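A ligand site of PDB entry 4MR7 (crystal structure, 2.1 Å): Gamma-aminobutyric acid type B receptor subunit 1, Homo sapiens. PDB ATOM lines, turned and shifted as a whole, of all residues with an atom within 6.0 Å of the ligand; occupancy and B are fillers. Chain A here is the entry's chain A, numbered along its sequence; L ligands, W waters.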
ATOM      1  N   GLY A  17      26.955 -17.218   9.210  1.00  0.00           N
ATOM      2  CA  GLY A  17      27.880 -17.175  10.348  1.00  0.00           C
ATOM      3  C   GLY A  17      27.679 -18.263  11.388  1.00  0.00           C
ATOM      4  O   GLY A  17      28.647 -18.920  11.795  1.00  0.00           O
ATOM      5  N   TRP A  18      26.431 -18.471  11.836  1.00  0.00           N
ATOM      6  CA  TRP A  18      26.125 -19.550  12.771  1.00  0.00           C
ATOM      7  C   TRP A  18      24.932 -20.303  12.167  1.00  0.00           C
ATOM      8  O   TRP A  18      23.806 -19.828  12.282  1.00  0.00           O
ATOM      9  CB  TRP A  18      25.814 -19.044  14.177  1.00  0.00           C
ATOM     10  CG  TRP A  18      25.394 -20.142  15.124  1.00  0.00           C
ATOM     11  CD1 TRP A  18      26.194 -21.101  15.666  1.00  0.00           C
ATOM     12  CD2 TRP A  18      24.079 -20.356  15.651  1.00  0.00           C
ATOM     13  NE1 TRP A  18      25.455 -21.922  16.493  1.00  0.00           N
ATOM     14  CE2 TRP A  18      24.151 -21.482  16.499  1.00  0.00           C
ATOM     15  CE3 TRP A  18      22.830 -19.733  15.452  1.00  0.00           C
ATOM     16  CZ2 TRP A  18      23.034 -21.981  17.184  1.00  0.00           C
ATOM     17  CZ3 TRP A  18      21.731 -20.196  16.158  1.00  0.00           C
ATOM     18  CH2 TRP A  18      21.834 -21.305  17.001  1.00  0.00           C
ATOM     19  N   CYS A  56      21.186 -16.524   8.727  1.00  0.00           N
ATOM     20  CA  CYS A  56      21.934 -15.761   9.741  1.00  0.00           C
ATOM     21  C   CYS A  56      22.181 -14.332   9.199  1.00  0.00           C
ATOM     22  O   CYS A  56      23.252 -13.744   9.402  1.00  0.00           O
ATOM     23  CB  CYS A  56      23.236 -16.488  10.079  1.00  0.00           C
ATOM     24  SG  CYS A  56      23.963 -16.063  11.680  1.00  0.00           S
ATOM     25  N   GLY A  81      17.050 -17.040  15.706  1.00  0.00           N
ATOM     26  CA  GLY A  81      18.258 -17.723  16.196  1.00  0.00           C
ATOM     27  C   GLY A  81      19.502 -16.859  16.407  1.00  0.00           C
ATOM     28  O   GLY A  81      19.960 -16.692  17.547  1.00  0.00           O
ATOM     29  N   CYS A  82      20.084 -16.338  15.289  1.00  0.00           N
ATOM     30  CA  CYS A  82      21.319 -15.529  15.268  1.00  0.00           C
ATOM     31  C   CYS A  82      21.097 -14.202  15.994  1.00  0.00           C
ATOM     32  O   CYS A  82      19.996 -13.652  15.929  1.00  0.00           O
ATOM     33  CB  CYS A  82      21.805 -15.311  13.831  1.00  0.00           C
ATOM     34  SG  CYS A  82      22.712 -16.746  13.152  1.00  0.00           S
ATOM     35  N   SER A  83      22.132 -13.675  16.645  1.00  0.00           N
ATOM     36  CA  SER A  83      22.089 -12.372  17.363  1.00  0.00           C
ATOM     37  C   SER A  83      21.750 -11.227  16.415  1.00  0.00           C
ATOM     38  O   SER A  83      20.918 -10.426  16.761  1.00  0.00           O
ATOM     39  CB  SER A  83      23.422 -12.088  18.037  1.00  0.00           C
ATOM     40  OG  SER A  83      23.483 -12.754  19.292  1.00  0.00           O
ATOM     41  N   SER A  84      22.346 -11.183  15.220  1.00  0.00           N
ATOM     42  CA  SER A  84      22.091 -10.121  14.242  1.00  0.00           C
ATOM     43  C   SER A  84      20.634 -10.168  13.826  1.00  0.00           C
ATOM     44  O   SER A  84      20.006  -9.129  13.695  1.00  0.00           O
ATOM     45  CB  SER A  84      23.006 -10.253  13.033  1.00  0.00           C
ATOM     46  OG  SER A  84      22.782 -11.485  12.362  1.00  0.00           O
ATOM     47  N   GLY A 104      19.238 -19.091  20.205  1.00  0.00           N
ATOM     48  CA  GLY A 104      20.666 -19.078  19.879  1.00  0.00           C
ATOM     49  C   GLY A 104      21.456 -17.798  20.034  1.00  0.00           C
ATOM     50  O   GLY A 104      22.658 -17.828  19.773  1.00  0.00           O
ATOM     51  N   SER A 105      20.856 -16.690  20.464  1.00  0.00           N
ATOM     52  CA  SER A 105      21.556 -15.389  20.552  1.00  0.00           C
ATOM     53  C   SER A 105      22.374 -15.150  21.810  1.00  0.00           C
ATOM     54  O   SER A 105      21.808 -15.095  22.903  1.00  0.00           O
ATOM     55  CB  SER A 105      20.545 -14.266  20.370  1.00  0.00           C
ATOM     56  OG  SER A 105      19.962 -14.372  19.086  1.00  0.00           O
ATOM     57  N   SER A 106      23.693 -14.902  21.652  1.00  0.00           N
ATOM     58  CA  SER A 106      24.621 -14.650  22.771  1.00  0.00           C
ATOM     59  C   SER A 106      24.984 -13.157  22.999  1.00  0.00           C
ATOM     60  O   SER A 106      25.675 -12.851  23.976  1.00  0.00           O
ATOM     61  CB  SER A 106      25.921 -15.421  22.542  1.00  0.00           C
ATOM     62  OG  SER A 106      26.469 -15.077  21.275  1.00  0.00           O
ATOM     63  N   SER A 107      24.634 -12.274  22.051  1.00  0.00           N
ATOM     64  CA  SER A 107      24.963 -10.856  22.101  1.00  0.00           C
ATOM     65  C   SER A 107      24.561 -10.157  23.415  1.00  0.00           C
ATOM     66  O   SER A 107      23.367 -10.048  23.722  1.00  0.00           O
ATOM     67  CB  SER A 107      24.396 -10.119  20.890  1.00  0.00           C
ATOM     68  OG  SER A 107      24.568  -8.718  20.983  1.00  0.00           O
ATOM     69  N   HIS A 123      19.229 -19.197  25.300  1.00  0.00           N
ATOM     70  CA  HIS A 123      20.681 -19.155  25.103  1.00  0.00           C
ATOM     71  C   HIS A 123      21.165 -18.032  26.034  1.00  0.00           C
ATOM     72  O   HIS A 123      20.626 -16.925  25.951  1.00  0.00           O
ATOM     73  CB  HIS A 123      21.053 -18.771  23.659  1.00  0.00           C
ATOM     74  CG  HIS A 123      22.516 -18.983  23.322  1.00  0.00           C
ATOM     75  ND1 HIS A 123      23.544 -18.307  23.992  1.00  0.00           N
ATOM     76  CD2 HIS A 123      23.086 -19.805  22.409  1.00  0.00           C
ATOM     77  CE1 HIS A 123      24.667 -18.728  23.461  1.00  0.00           C
ATOM     78  NE2 HIS A 123      24.440 -19.645  22.516  1.00  0.00           N
ATOM     79  N   PRO A 124      22.171 -18.244  26.875  1.00  0.00           N
ATOM     80  CA  PRO A 124      22.641 -17.129  27.712  1.00  0.00           C
ATOM     81  C   PRO A 124      23.414 -16.062  26.931  1.00  0.00           C
ATOM     82  O   PRO A 124      23.863 -16.261  25.785  1.00  0.00           O
ATOM     83  CB  PRO A 124      23.621 -17.829  28.685  1.00  0.00           C
ATOM     84  CG  PRO A 124      23.275 -19.258  28.626  1.00  0.00           C
ATOM     85  CD  PRO A 124      22.915 -19.473  27.185  1.00  0.00           C
ATOM     86  N   TYR A 203      37.714 -14.586  18.201  1.00  0.00           N
ATOM     87  CA  TYR A 203      37.274 -15.783  17.507  1.00  0.00           C
ATOM     88  C   TYR A 203      38.487 -16.686  17.276  1.00  0.00           C
ATOM     89  O   TYR A 203      39.609 -16.267  17.572  1.00  0.00           O
ATOM     90  CB  TYR A 203      36.519 -15.443  16.214  1.00  0.00           C
ATOM     91  CG  TYR A 203      35.150 -14.899  16.535  1.00  0.00           C
ATOM     92  CD1 TYR A 203      34.229 -15.665  17.248  1.00  0.00           C
ATOM     93  CD2 TYR A 203      34.805 -13.592  16.203  1.00  0.00           C
ATOM     94  CE1 TYR A 203      32.982 -15.151  17.604  1.00  0.00           C
ATOM     95  CE2 TYR A 203      33.553 -13.070  16.559  1.00  0.00           C
ATOM     96  CZ  TYR A 203      32.640 -13.858  17.238  1.00  0.00           C
ATOM     97  OH  TYR A 203      31.422 -13.338  17.597  1.00  0.00           O
ATOM     98  N   TRP A 231      34.486 -22.368  23.259  1.00  0.00           N
ATOM     99  CA  TRP A 231      33.722 -22.998  22.172  1.00  0.00           C
ATOM    100  C   TRP A 231      34.482 -23.093  20.866  1.00  0.00           C
ATOM    101  O   TRP A 231      33.873 -23.336  19.822  1.00  0.00           O
ATOM    102  CB  TRP A 231      32.325 -22.391  21.980  1.00  0.00           C
ATOM    103  CG  TRP A 231      32.223 -20.909  22.133  1.00  0.00           C
ATOM    104  CD1 TRP A 231      31.562 -20.236  23.123  1.00  0.00           C
ATOM    105  CD2 TRP A 231      32.716 -19.927  21.222  1.00  0.00           C
ATOM    106  NE1 TRP A 231      31.635 -18.883  22.896  1.00  0.00           N
ATOM    107  CE2 TRP A 231      32.337 -18.658  21.729  1.00  0.00           C
ATOM    108  CE3 TRP A 231      33.457 -19.986  20.019  1.00  0.00           C
ATOM    109  CZ2 TRP A 231      32.630 -17.474  21.056  1.00  0.00           C
ATOM    110  CZ3 TRP A 231      33.753 -18.810  19.361  1.00  0.00           C
ATOM    111  CH2 TRP A 231      33.347 -17.566  19.889  1.00  0.00           C
ATOM    112  N   ILE A 263      29.342 -22.299  28.243  1.00  0.00           N
ATOM    113  CA  ILE A 263      28.018 -22.528  28.785  1.00  0.00           C
ATOM    114  C   ILE A 263      27.629 -24.001  28.660  1.00  0.00           C
ATOM    115  O   ILE A 263      27.927 -24.644  27.645  1.00  0.00           O
ATOM    116  CB  ILE A 263      26.984 -21.539  28.167  1.00  0.00           C
ATOM    117  CG1 ILE A 263      27.259 -20.110  28.681  1.00  0.00           C
ATOM    118  CG2 ILE A 263      25.537 -21.962  28.457  1.00  0.00           C
ATOM    119  CD1 ILE A 263      27.265 -19.060  27.588  1.00  0.00           C
ATOM    120  N   MET A 265      25.127 -26.583  27.965  1.00  0.00           N
ATOM    121  CA  MET A 265      23.935 -26.596  27.112  1.00  0.00           C
ATOM    122  C   MET A 265      23.132 -27.892  27.177  1.00  0.00           C
ATOM    123  O   MET A 265      22.015 -27.936  26.688  1.00  0.00           O
ATOM    124  CB  MET A 265      24.342 -26.272  25.675  1.00  0.00           C
ATOM    125  CG  MET A 265      24.611 -24.811  25.503  1.00  0.00           C
ATOM    126  SD  MET A 265      25.087 -24.452  23.822  1.00  0.00           S
ATOM    127  CE  MET A 265      25.429 -22.664  23.988  1.00  0.00           C
ATOM    128  N   GLN A 301      25.041 -28.434  19.428  1.00  0.00           N
ATOM    129  CA  GLN A 301      25.183 -28.184  20.859  1.00  0.00           C
ATOM    130  C   GLN A 301      24.111 -27.265  21.423  1.00  0.00           C
ATOM    131  O   GLN A 301      23.771 -27.382  22.606  1.00  0.00           O
ATOM    132  CB  GLN A 301      26.595 -27.692  21.230  1.00  0.00           C
ATOM    133  CG  GLN A 301      27.066 -26.450  20.465  1.00  0.00           C
ATOM    134  CD  GLN A 301      28.275 -25.743  21.095  1.00  0.00           C
ATOM    135  OE1 GLN A 301      28.945 -26.271  21.998  1.00  0.00           O
ATOM    136  NE2 GLN A 301      28.586 -24.539  20.601  1.00  0.00           N
ATOM    137  N   GLU A 302      23.596 -26.337  20.584  1.00  0.00           N
ATOM    138  CA  GLU A 302      22.552 -25.394  21.007  1.00  0.00           C
ATOM    139  C   GLU A 302      21.182 -25.990  20.931  1.00  0.00           C
ATOM    140  O   GLU A 302      20.271 -25.405  21.516  1.00  0.00           O
ATOM    141  CB  GLU A 302      22.601 -24.088  20.203  1.00  0.00           C
ATOM    142  CG  GLU A 302      23.798 -23.226  20.530  1.00  0.00           C
ATOM    143  CD  GLU A 302      25.036 -23.577  19.729  1.00  0.00           C
ATOM    144  OE1 GLU A 302      24.952 -24.419  18.816  1.00  0.00           O
ATOM    145  OE2 GLU A 302      26.095 -22.976  20.001  1.00  0.00           O
HETATM  146  O1  LIG L   1      25.000 -14.957  18.962  1.00  0.00           O
HETATM  147  P1  LIG L   1      25.423 -15.602  17.711  1.00  0.00           P
HETATM  148  O2  LIG L   1      24.467 -15.035  16.577  1.00  0.00           O
HETATM  149  C1  LIG L   1      27.164 -15.262  17.334  1.00  0.00           C
HETATM  150  C2  LIG L   1      27.711 -16.083  16.141  1.00  0.00           C
HETATM  151  C3  LIG L   1      27.725 -15.287  14.829  1.00  0.00           C
HETATM  152  C4  LIG L   1      29.065 -15.202  14.070  1.00  0.00           C
HETATM  153  C5  LIG L   1      29.914 -16.488  14.067  1.00  0.00           C
HETATM  154  C6  LIG L   1      29.817 -17.336  15.345  1.00  0.00           C
HETATM  155  C7  LIG L   1      29.072 -16.679  16.513  1.00  0.00           C
HETATM  156  C8  LIG L   1      25.138 -17.393  17.828  1.00  0.00           C
HETATM  157  C9  LIG L   1      25.789 -17.997  19.069  1.00  0.00           C
HETATM  158  O3  LIG L   1      25.261 -17.451  20.300  1.00  0.00           O
HETATM  159  C10 LIG L   1      25.527 -19.508  19.087  1.00  0.00           C
HETATM  160  N1  LIG L   1      26.105 -20.149  20.265  1.00  0.00           N
HETATM  161  C11 LIG L   1      27.473 -19.903  20.746  1.00  0.00           C
HETATM  162  C12 LIG L   1      27.828 -20.651  22.021  1.00  0.00           C
HETATM  163  C13 LIG L   1      28.520 -20.068  19.701  1.00  0.00           C
HETATM  164  C14 LIG L   1      29.533 -19.102  19.648  1.00  0.00           C
HETATM  165  C15 LIG L   1      30.554 -19.165  18.702  1.00  0.00           C
HETATM  166  C16 LIG L   1      30.599 -20.242  17.822  1.00  0.00           C
HETATM  167 CL1  LIG L   1      31.879 -20.446  16.575  1.00  0.00          CL
HETATM  168  C17 LIG L   1      29.527 -21.264  17.893  1.00  0.00           C
HETATM  169 CL2  LIG L   1      29.582 -22.590  16.709  1.00  0.00          CL
HETATM  170  C18 LIG L   1      28.504 -21.168  18.823  1.00  0.00           C
HETATM  171  O   HOH W   1      34.988 -21.723  16.253  1.00  0.00           O
HETATM  172  O   HOH W   2      29.208 -23.451  13.795  1.00  0.00           O
HETATM  173  O   HOH W   3      24.708 -13.062  14.657  1.00  0.00           O
HETATM  174  O   HOH W   4      32.289 -19.747  13.657  1.00  0.00           O
HETATM  175  O   HOH W   5      27.491 -12.784  20.099  1.00  0.00           O
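O of Gly 104 is in hydrogen-bond range of O3 of the ligand (2.7 Å). An oxygen (O2) of the ligand lies within hydrogen-bond range of the backbone NH (N) of Ser 83 (2.7 Å). OG of Ser 83 sits at hydrogen-bond distance from O1 of the ligand. The backbone NH (N) of Ser 106 sits at hydrogen-bond distance from an oxygen (O1) of the ligand (3.0 Å). An oxygen (O1) of the ligand is in hydrogen-bond range of the side-chain hydroxyl of Ser 106, 2.7 Å away. The side-chain carboxylate (OE2) of Glu 302 lies within salt-bridge range of a nitrogen (N1) of the ligand, at 2.8 Å. N1 of the ligand is in hydrogen-bond range of NE2 of His 123 (2.8 Å).
The side-chain hydroxyl of Ser 83 is in hydrogen-bond range of the backbone NH of Ser 106 (3.2 Å). The backbone NH (N) of Ser 83 is in hydrogen-bond range of the side-chain hydroxyl (OG) of Ser 105 (3.3 Å). OG of Ser 83 lies within hydrogen-bond range of N of Ser 107 (3.0 Å). The indole nitrogen of Trp 18 is in hydrogen-bond range of the side-chain carboxylate of Glu 302 (3.4 Å). The side-chain carboxylate (OE2) of Glu 302 is in hydrogen-bond range of the side-chain amide nitrogen (NE2) of Gln 301 (3.0 Å). The backbone carbonyl oxygen of Cys 82 sits at hydrogen-bond distance from the side-chain hydroxyl of Ser 105 (3.2 Å). SG of Cys 82 is disulfide-bonded to SG of Cys 56. The backbone NH (N) of Trp 18 is in hydrogen-bond range of the side-chain sulfur (SG) of Cys 56 (3.5 Å).
Gly 17 touches the ligand (O to C5, 3.6 Å). Trp 18 touches the ligand (CE2 to C10, 3.5 Å). CA of Cys 82 touches O2 of the ligand (3.4 Å). Ser 105 touches the ligand. Trp 231 touches the ligand (CZ3 to C15, 3.3 Å). Met 265 touches the ligand. Gln 301 touches the ligand (NE2 to C18, 3.8 Å). Hydrophobic or aromatic side chains within 4 Å of the ligand: Trp 18, His 123, Trp 231 and Met 265. The nearest printed residue that does not touch the ligand is Ser 107 (4.1 Å).
Water W3 lies within hydrogen-bond range of O2 of the ligand (2.8 Å), N of Ser 84 (3.1 Å) and N of Ser 83 (3.3 Å). Water W5 lies within hydrogen-bond range of the side-chain hydroxyl (OG) of Ser 106 (2.8 Å), an oxygen (O1) of the ligand (3.5 Å) and the backbone NH (N) of Ser 107 (3.5 Å).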
